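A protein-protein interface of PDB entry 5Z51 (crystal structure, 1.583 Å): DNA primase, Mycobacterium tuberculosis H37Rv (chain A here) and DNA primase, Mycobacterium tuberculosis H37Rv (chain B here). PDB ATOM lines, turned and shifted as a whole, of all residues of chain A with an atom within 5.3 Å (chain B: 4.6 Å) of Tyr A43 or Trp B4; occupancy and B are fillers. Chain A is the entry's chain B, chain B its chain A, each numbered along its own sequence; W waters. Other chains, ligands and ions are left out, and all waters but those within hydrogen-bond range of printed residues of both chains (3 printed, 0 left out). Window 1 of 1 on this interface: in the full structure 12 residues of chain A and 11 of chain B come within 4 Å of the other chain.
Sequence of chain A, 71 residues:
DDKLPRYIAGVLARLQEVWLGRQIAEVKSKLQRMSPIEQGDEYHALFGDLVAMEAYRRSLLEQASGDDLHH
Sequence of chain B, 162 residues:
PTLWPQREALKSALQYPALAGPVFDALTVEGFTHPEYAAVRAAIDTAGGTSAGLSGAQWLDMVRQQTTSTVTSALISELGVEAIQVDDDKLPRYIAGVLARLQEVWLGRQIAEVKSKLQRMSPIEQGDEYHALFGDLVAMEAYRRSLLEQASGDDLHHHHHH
Among the printed residues, pairs that only touch across the chains: Ser A35 with His B159, Pro A36 with His B157, His A44 with Leu B3, Tyr A43 with Trp B4, Pro A36 with Trp B4, Phe A47 with Arg B7, Pro A36 with His B159, Tyr A43 with His B157, Phe A47 with Trp B4, His A44 with Trp B4, Leu A31 with His B159 and Gly A40 with Trp B4.
Water W3 lies within hydrogen-bond range of OE1 of Gln B85 (2.6 Å), OH of Tyr A43 (2.8 Å) and NE2 of His B157 (2.9 Å). Water W2 bridges O of His B159 (2.7 Å) and N of Met A34 (3.4 Å). Water W1 lies within hydrogen-bond range of N of Trp B4, OD1 of Asp A41 and N of Leu B3.
Printed residues of chain B within 4 Å of Tyr A43: Trp B4 (3.6 Å), His B157 (3.8 Å) and His B159 (2.5 Å). Of chain A, only Pro A36, Gly A40, Tyr A43, His A44 and Phe A47 come within 4 Å of Trp B4. Of the printed residues of chain B, His A44 touches Leu B3 and Trp B4. Of the printed residues of chain A, His B159 touches Leu A31, Met A34, Ser A35, Pro A36 and Tyr A43. Of the printed residues of chain B, Pro A36 touches Trp B4, His B157 and His B159. Of the printed residues of chain B, Ser A35 touches His B159 (3.4 Å). Glu B8 touches none of the printed residues of chain A. The nearest residue of chain A that does not touch Trp B4 is Asp A41 (5.1 Å).
Hydrophobic or aromatic side chains of chain A within 4 Å of the printed part of chain B: Pro A36, Tyr A43, His A44 and Phe A47. Along chain A the printed residues that touch a printed residue of chain B span positions 31 to 47. Of the 11 printed residues of chain B, 5 touch a printed residue of chain A. Along chain B the printed residues that touch a printed residue of chain A span positions 3 to 159. Among the printed residues, 14 pairs touch across the chains.
A ring nitrogen (ND1) of His B157 lies within hydrogen-bond range of the backbone NH of His B159, 2.8 Å away. The side-chain amide oxygen (OE1) of Gln A39 lies within hydrogen-bond range of the backbone NH (N) of Ser A35 (3.3 Å).
ND1 of His B159 is in hydrogen-bond range of OH of Tyr A43 (2.5 Å). O of Met A34 lies close to O of His B159, at 3.3 Å.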
ATOM      1  N   LEU A  31       7.972  -1.629 -33.480  1.00  0.00           N
ATOM      2  CA  LEU A  31       8.426  -2.391 -32.307  1.00  0.00           C
ATOM      3  C   LEU A  31       7.514  -3.584 -32.043  1.00  0.00           C
ATOM      4  O   LEU A  31       7.987  -4.650 -31.652  1.00  0.00           O
ATOM      5  CB  LEU A  31       8.481  -1.509 -31.038  1.00  0.00           C
ATOM      6  CG  LEU A  31       9.667  -0.542 -31.040  1.00  0.00           C
ATOM      7  CD1 LEU A  31       9.316   0.591 -30.094  1.00  0.00           C
ATOM      8  CD2 LEU A  31      10.927  -1.334 -30.577  1.00  0.00           C
ATOM      9  N   MET A  34       8.724  -6.693 -33.780  1.00  0.00           N
ATOM     10  CA  MET A  34      10.110  -7.117 -33.453  1.00  0.00           C
ATOM     11  C   MET A  34      10.165  -7.749 -32.075  1.00  0.00           C
ATOM     12  O   MET A  34       9.563  -7.277 -31.120  1.00  0.00           O
ATOM     13  CB  MET A  34      11.070  -5.932 -33.420  1.00  0.00           C
ATOM     14  CG  MET A  34      10.990  -5.094 -34.687  1.00  0.00           C
ATOM     15  SD  MET A  34      11.961  -3.434 -34.430  1.00  0.00           S
ATOM     16  CE  MET A  34      13.559  -4.340 -33.602  1.00  0.00           C
ATOM     17  N   SER A  35      10.928  -8.813 -31.951  1.00  0.00           N
ATOM     18  CA  SER A  35      11.074  -9.468 -30.667  1.00  0.00           C
ATOM     19  C   SER A  35      12.247  -8.890 -29.888  1.00  0.00           C
ATOM     20  O   SER A  35      13.350  -8.776 -30.417  1.00  0.00           O
ATOM     21  CB  SER A  35      11.317 -10.973 -30.901  1.00  0.00           C
ATOM     22  OG  SER A  35      11.839 -11.535 -29.694  1.00  0.00           O
ATOM     23  N   PRO A  36      12.023  -8.479 -28.636  1.00  0.00           N
ATOM     24  CA  PRO A  36      13.205  -8.047 -27.872  1.00  0.00           C
ATOM     25  C   PRO A  36      14.128  -9.168 -27.406  1.00  0.00           C
ATOM     26  O   PRO A  36      15.157  -8.880 -26.761  1.00  0.00           O
ATOM     27  CB  PRO A  36      12.605  -7.335 -26.668  1.00  0.00           C
ATOM     28  CG  PRO A  36      11.230  -7.912 -26.518  1.00  0.00           C
ATOM     29  CD  PRO A  36      10.756  -8.296 -27.886  1.00  0.00           C
ATOM     30  N   GLN A  39      15.903  -9.855 -31.174  1.00  0.00           N
ATOM     31  CA  GLN A  39      16.572  -8.668 -31.671  1.00  0.00           C
ATOM     32  C   GLN A  39      16.668  -7.639 -30.555  1.00  0.00           C
ATOM     33  O   GLN A  39      16.294  -6.496 -30.767  1.00  0.00           O
ATOM     34  CB  GLN A  39      15.763  -8.054 -32.814  1.00  0.00           C
ATOM     35  CG  GLN A  39      15.569  -8.969 -34.037  1.00  0.00           C
ATOM     36  CD  GLN A  39      14.301  -8.597 -34.810  1.00  0.00           C
ATOM     37  OE1 GLN A  39      13.174  -8.909 -34.385  1.00  0.00           O
ATOM     38  NE2 GLN A  39      14.477  -7.910 -35.921  1.00  0.00           N
ATOM     39  N   GLY A  40      17.169  -8.040 -29.392  1.00  0.00           N
ATOM     40  CA  GLY A  40      17.225  -7.189 -28.203  1.00  0.00           C
ATOM     41  C   GLY A  40      17.903  -5.865 -28.478  1.00  0.00           C
ATOM     42  O   GLY A  40      17.416  -4.828 -28.052  1.00  0.00           O
ATOM     43  N   ASP A  41      19.055  -5.870 -29.138  1.00  0.00           N
ATOM     44  CA  ASP A  41      19.804  -4.634 -29.304  1.00  0.00           C
ATOM     45  C   ASP A  41      19.091  -3.685 -30.253  1.00  0.00           C
ATOM     46  O   ASP A  41      19.046  -2.476 -29.984  1.00  0.00           O
ATOM     47  CB  ASP A  41      21.198  -4.921 -29.848  1.00  0.00           C
ATOM     48  CG  ASP A  41      22.113  -5.479 -28.793  1.00  0.00           C
ATOM     49  OD1 ASP A  41      21.772  -5.407 -27.574  1.00  0.00           O
ATOM     50  OD2 ASP A  41      23.168  -6.003 -29.205  1.00  0.00           O
ATOM     51  N   GLU A  42      18.535  -4.216 -31.344  1.00  0.00           N
ATOM     52  CA  GLU A  42      17.807  -3.345 -32.280  1.00  0.00           C
ATOM     53  C   GLU A  42      16.552  -2.807 -31.637  1.00  0.00           C
ATOM     54  O   GLU A  42      16.194  -1.633 -31.850  1.00  0.00           O
ATOM     55  CB  GLU A  42      17.409  -4.102 -33.538  1.00  0.00           C
ATOM     56  CG  GLU A  42      18.596  -4.359 -34.500  1.00  0.00           C
ATOM     57  CD  GLU A  42      18.182  -5.241 -35.632  1.00  0.00           C
ATOM     58  OE1 GLU A  42      17.417  -4.760 -36.504  1.00  0.00           O
ATOM     59  OE2 GLU A  42      18.569  -6.431 -35.626  1.00  0.00           O
ATOM     60  N   TYR A  43      15.871  -3.685 -30.910  1.00  0.00           N
ATOM     61  CA  TYR A  43      14.634  -3.341 -30.232  1.00  0.00           C
ATOM     62  C   TYR A  43      14.950  -2.284 -29.192  1.00  0.00           C
ATOM     63  O   TYR A  43      14.294  -1.220 -29.161  1.00  0.00           O
ATOM     64  CB  TYR A  43      14.034  -4.594 -29.590  1.00  0.00           C
ATOM     65  CG  TYR A  43      12.687  -4.350 -28.995  1.00  0.00           C
ATOM     66  CD1 TYR A  43      12.565  -3.681 -27.782  1.00  0.00           C
ATOM     67  CD2 TYR A  43      11.525  -4.802 -29.651  1.00  0.00           C
ATOM     68  CE1 TYR A  43      11.291  -3.452 -27.218  1.00  0.00           C
ATOM     69  CE2 TYR A  43      10.282  -4.599 -29.085  1.00  0.00           C
ATOM     70  CZ  TYR A  43      10.183  -3.925 -27.879  1.00  0.00           C
ATOM     71  OH  TYR A  43       8.954  -3.704 -27.323  1.00  0.00           O
ATOM     72  N   HIS A  44      15.975  -2.504 -28.379  1.00  0.00           N
ATOM     73  CA  HIS A  44      16.329  -1.495 -27.360  1.00  0.00           C
ATOM     74  C   HIS A  44      16.644  -0.143 -27.976  1.00  0.00           C
ATOM     75  O   HIS A  44      16.251   0.901 -27.448  1.00  0.00           O
ATOM     76  CB  HIS A  44      17.570  -1.993 -26.575  1.00  0.00           C
ATOM     77  CG  HIS A  44      18.049  -1.002 -25.545  1.00  0.00           C
ATOM     78  ND1 HIS A  44      19.019  -0.071 -25.818  1.00  0.00           N
ATOM     79  CD2 HIS A  44      17.636  -0.776 -24.267  1.00  0.00           C
ATOM     80  CE1 HIS A  44      19.200   0.698 -24.744  1.00  0.00           C
ATOM     81  NE2 HIS A  44      18.382   0.285 -23.791  1.00  0.00           N
ATOM     82  N   ALA A  45      17.403  -0.140 -29.071  1.00  0.00           N
ATOM     83  CA  ALA A  45      17.794   1.085 -29.730  1.00  0.00           C
ATOM     84  C   ALA A  45      16.571   1.874 -30.206  1.00  0.00           C
ATOM     85  O   ALA A  45      16.439   3.109 -29.959  1.00  0.00           O
ATOM     86  CB  ALA A  45      18.725   0.748 -30.904  1.00  0.00           C
ATOM     87  N   LEU A  46      15.690   1.156 -30.897  1.00  0.00           N
ATOM     88  CA  LEU A  46      14.499   1.830 -31.435  1.00  0.00           C
ATOM     89  C   LEU A  46      13.583   2.291 -30.282  1.00  0.00           C
ATOM     90  O   LEU A  46      13.031   3.413 -30.319  1.00  0.00           O
ATOM     91  CB  LEU A  46      13.766   0.859 -32.366  1.00  0.00           C
ATOM     92  CG  LEU A  46      12.464   1.408 -32.972  1.00  0.00           C
ATOM     93  CD1 LEU A  46      12.753   2.708 -33.747  1.00  0.00           C
ATOM     94  CD2 LEU A  46      11.879   0.346 -33.904  1.00  0.00           C
ATOM     95  N   PHE A  47      13.422   1.437 -29.275  1.00  0.00           N
ATOM     96  CA  PHE A  47      12.624   1.799 -28.110  1.00  0.00           C
ATOM     97  C   PHE A  47      13.168   3.045 -27.440  1.00  0.00           C
ATOM     98  O   PHE A  47      12.396   3.927 -27.021  1.00  0.00           O
ATOM     99  CB  PHE A  47      12.614   0.626 -27.140  1.00  0.00           C
ATOM    100  CG  PHE A  47      11.600   0.760 -26.049  1.00  0.00           C
ATOM    101  CD1 PHE A  47      11.921   1.445 -24.899  1.00  0.00           C
ATOM    102  CD2 PHE A  47      10.368   0.159 -26.172  1.00  0.00           C
ATOM    103  CE1 PHE A  47      10.980   1.585 -23.851  1.00  0.00           C
ATOM    104  CE2 PHE A  47       9.405   0.297 -25.135  1.00  0.00           C
ATOM    105  CZ  PHE A  47       9.730   1.017 -23.976  1.00  0.00           C
ATOM    106  N   GLY A  48      14.479   3.164 -27.332  1.00  0.00           N
ATOM    107  CA  GLY A  48      15.066   4.361 -26.743  1.00  0.00           C
ATOM    108  C   GLY A  48      14.640   5.617 -27.482  1.00  0.00           C
ATOM    109  O   GLY A  48      14.312   6.665 -26.860  1.00  0.00           O
ATOM    110  N   THR B   2      23.426  -6.986 -23.619  1.00  0.00           N
ATOM    111  CA  THR B   2      22.426  -7.064 -22.606  1.00  0.00           C
ATOM    112  C   THR B   2      21.702  -5.767 -22.392  1.00  0.00           C
ATOM    113  O   THR B   2      21.159  -5.565 -21.394  1.00  0.00           O
ATOM    114  CB  THR B   2      23.093  -7.454 -21.275  1.00  0.00           C
ATOM    115  OG1 THR B   2      24.161  -6.593 -20.982  1.00  0.00           O
ATOM    116  CG2 THR B   2      23.627  -8.850 -21.371  1.00  0.00           C
ATOM    117  N   LEU B   3      21.700  -4.893 -23.394  1.00  0.00           N
ATOM    118  CA  LEU B   3      21.056  -3.619 -23.132  1.00  0.00           C
ATOM    119  C   LEU B   3      19.570  -3.707 -22.801  1.00  0.00           C
ATOM    120  O   LEU B   3      19.097  -2.991 -21.902  1.00  0.00           O
ATOM    121  CB  LEU B   3      21.225  -2.638 -24.319  1.00  0.00           C
ATOM    122  CG  LEU B   3      22.659  -2.128 -24.443  1.00  0.00           C
ATOM    123  CD1 LEU B   3      22.830  -1.399 -25.798  1.00  0.00           C
ATOM    124  CD2 LEU B   3      22.954  -1.183 -23.313  1.00  0.00           C
ATOM    125  N   TRP B   4      18.827  -4.524 -23.546  1.00  0.00           N
ATOM    126  CA  TRP B   4      17.382  -4.696 -23.240  1.00  0.00           C
ATOM    127  C   TRP B   4      17.191  -5.251 -21.811  1.00  0.00           C
ATOM    128  O   TRP B   4      16.498  -4.635 -20.973  1.00  0.00           O
ATOM    129  CB  TRP B   4      16.627  -5.545 -24.282  1.00  0.00           C
ATOM    130  CG  TRP B   4      15.149  -5.508 -23.962  1.00  0.00           C
ATOM    131  CD1 TRP B   4      14.360  -6.569 -23.510  1.00  0.00           C
ATOM    132  CD2 TRP B   4      14.281  -4.357 -23.974  1.00  0.00           C
ATOM    133  NE1 TRP B   4      13.068  -6.144 -23.302  1.00  0.00           N
ATOM    134  CE2 TRP B   4      12.994  -4.793 -23.547  1.00  0.00           C
ATOM    135  CE3 TRP B   4      14.455  -3.001 -24.327  1.00  0.00           C
ATOM    136  CZ2 TRP B   4      11.885  -3.918 -23.478  1.00  0.00           C
ATOM    137  CZ3 TRP B   4      13.376  -2.117 -24.237  1.00  0.00           C
ATOM    138  CH2 TRP B   4      12.086  -2.596 -23.826  1.00  0.00           C
ATOM    139  N   PRO B   5      17.841  -6.396 -21.440  1.00  0.00           N
ATOM    140  CA  PRO B   5      17.619  -6.803 -20.033  1.00  0.00           C
ATOM    141  C   PRO B   5      18.164  -5.845 -18.975  1.00  0.00           C
ATOM    142  O   PRO B   5      17.602  -5.824 -17.886  1.00  0.00           O
ATOM    143  CB  PRO B   5      18.321  -8.171 -19.913  1.00  0.00           C
ATOM    144  CG  PRO B   5      19.122  -8.325 -21.170  1.00  0.00           C
ATOM    145  CD  PRO B   5      18.580  -7.383 -22.232  1.00  0.00           C
ATOM    146  N   GLN B   6      19.213  -5.068 -19.272  1.00  0.00           N
ATOM    147  CA  GLN B   6      19.611  -4.010 -18.325  1.00  0.00           C
ATOM    148  C   GLN B   6      18.470  -3.046 -18.050  1.00  0.00           C
ATOM    149  O   GLN B   6      18.185  -2.750 -16.906  1.00  0.00           O
ATOM    150  CB  GLN B   6      20.790  -3.180 -18.845  1.00  0.00           C
ATOM    151  CG  GLN B   6      22.139  -3.924 -18.833  1.00  0.00           C
ATOM    152  CD  GLN B   6      23.197  -3.079 -19.535  1.00  0.00           C
ATOM    153  OE1 GLN B   6      23.344  -1.865 -19.264  1.00  0.00           O
ATOM    154  NE2 GLN B   6      23.947  -3.704 -20.420  1.00  0.00           N
ATOM    155  N   ARG B   7      17.815  -2.556 -19.095  1.00  0.00           N
ATOM    156  CA  ARG B   7      16.687  -1.627 -18.867  1.00  0.00           C
ATOM    157  C   ARG B   7      15.555  -2.313 -18.104  1.00  0.00           C
ATOM    158  O   ARG B   7      15.000  -1.750 -17.172  1.00  0.00           O
ATOM    159  CB  ARG B   7      16.167  -1.151 -20.227  1.00  0.00           C
ATOM    160  CG  ARG B   7      15.133  -0.025 -20.101  1.00  0.00           C
ATOM    161  CD  ARG B   7      14.593   0.359 -21.481  1.00  0.00           C
ATOM    162  NE  ARG B   7      13.669   1.525 -21.399  1.00  0.00           N
ATOM    163  CZ  ARG B   7      14.063   2.802 -21.379  1.00  0.00           C
ATOM    164  NH1 ARG B   7      15.347   3.135 -21.507  1.00  0.00           N
ATOM    165  NH2 ARG B   7      13.146   3.765 -21.334  1.00  0.00           N
ATOM    166  N   GLU B   8      15.225  -3.552 -18.494  1.00  0.00           N
ATOM    167  CA  GLU B   8      14.127  -4.248 -17.828  1.00  0.00           C
ATOM    168  C   GLU B   8      14.490  -4.533 -16.367  1.00  0.00           C
ATOM    169  O   GLU B   8      13.595  -4.489 -15.489  1.00  0.00           O
ATOM    170  CB  GLU B   8      13.825  -5.572 -18.581  1.00  0.00           C
ATOM    171  CG  GLU B   8      13.284  -5.362 -20.013  1.00  0.00           C
ATOM    172  CD  GLU B   8      11.902  -4.721 -20.005  1.00  0.00           C
ATOM    173  OE1 GLU B   8      10.879  -5.421 -20.062  1.00  0.00           O
ATOM    174  OE2 GLU B   8      11.855  -3.495 -19.936  1.00  0.00           O
ATOM    175  N   GLN B  85       6.117  -5.001 -20.130  1.00  0.00           N
ATOM    176  CA  GLN B  85       5.036  -5.504 -21.004  1.00  0.00           C
ATOM    177  C   GLN B  85       4.999  -7.036 -20.940  1.00  0.00           C
ATOM    178  O   GLN B  85       5.607  -7.752 -21.788  1.00  0.00           O
ATOM    179  CB  GLN B  85       5.160  -4.974 -22.447  1.00  0.00           C
ATOM    180  CG  GLN B  85       5.119  -3.444 -22.537  1.00  0.00           C
ATOM    181  CD  GLN B  85       5.084  -2.963 -23.967  1.00  0.00           C
ATOM    182  OE1 GLN B  85       6.056  -2.413 -24.485  1.00  0.00           O
ATOM    183  NE2 GLN B  85       3.940  -3.137 -24.610  1.00  0.00           N
ATOM    184  N   TYR B  94       9.365 -13.474 -15.312  1.00  0.00           N
ATOM    185  CA  TYR B  94       9.919 -12.560 -16.305  1.00  0.00           C
ATOM    186  C   TYR B  94      11.076 -11.822 -15.668  1.00  0.00           C
ATOM    187  O   TYR B  94      12.170 -11.730 -16.268  1.00  0.00           O
ATOM    188  CB  TYR B  94       8.841 -11.594 -16.834  1.00  0.00           C
ATOM    189  CG  TYR B  94       9.413 -10.604 -17.791  1.00  0.00           C
ATOM    190  CD1 TYR B  94       9.595 -10.940 -19.138  1.00  0.00           C
ATOM    191  CD2 TYR B  94       9.761  -9.320 -17.368  1.00  0.00           C
ATOM    192  CE1 TYR B  94      10.168 -10.030 -20.021  1.00  0.00           C
ATOM    193  CE2 TYR B  94      10.335  -8.397 -18.243  1.00  0.00           C
ATOM    194  CZ  TYR B  94      10.501  -8.750 -19.578  1.00  0.00           C
ATOM    195  OH  TYR B  94      11.062  -7.887 -20.494  1.00  0.00           O
ATOM    196  N   HIS B 157       7.831 -11.923 -22.721  1.00  0.00           N
ATOM    197  CA  HIS B 157       7.564 -10.524 -23.155  1.00  0.00           C
ATOM    198  C   HIS B 157       6.440 -10.459 -24.202  1.00  0.00           C
ATOM    199  O   HIS B 157       6.347 -11.306 -25.094  1.00  0.00           O
ATOM    200  CB  HIS B 157       8.830  -9.837 -23.692  1.00  0.00           C
ATOM    201  CG  HIS B 157       8.683  -8.353 -23.860  1.00  0.00           C
ATOM    202  ND1 HIS B 157       8.108  -7.787 -24.976  1.00  0.00           N
ATOM    203  CD2 HIS B 157       9.021  -7.314 -23.045  1.00  0.00           C
ATOM    204  CE1 HIS B 157       8.107  -6.466 -24.856  1.00  0.00           C
ATOM    205  NE2 HIS B 157       8.684  -6.151 -23.703  1.00  0.00           N
ATOM    206  N   HIS B 159       6.092  -8.724 -26.737  1.00  0.00           N
ATOM    207  CA  HIS B 159       6.503  -8.582 -28.136  1.00  0.00           C
ATOM    208  C   HIS B 159       7.328  -9.754 -28.658  1.00  0.00           C
ATOM    209  O   HIS B 159       7.752  -9.725 -29.833  1.00  0.00           O
ATOM    210  CB  HIS B 159       7.214  -7.245 -28.324  1.00  0.00           C
ATOM    211  CG  HIS B 159       6.291  -6.070 -28.142  1.00  0.00           C
ATOM    212  ND1 HIS B 159       6.729  -4.777 -27.944  1.00  0.00           N
ATOM    213  CD2 HIS B 159       4.930  -6.011 -28.127  1.00  0.00           C
ATOM    214  CE1 HIS B 159       5.683  -3.973 -27.792  1.00  0.00           C
ATOM    215  NE2 HIS B 159       4.576  -4.693 -27.915  1.00  0.00           N
HETATM  216  O   HOH W   1      19.730  -6.205 -25.668  1.00  0.00           O
HETATM  217  O   HOH W   2       7.050  -9.266 -32.348  1.00  0.00           O
HETATM  218  O   HOH W   3       8.461  -3.408 -24.533  1.00  0.00           O
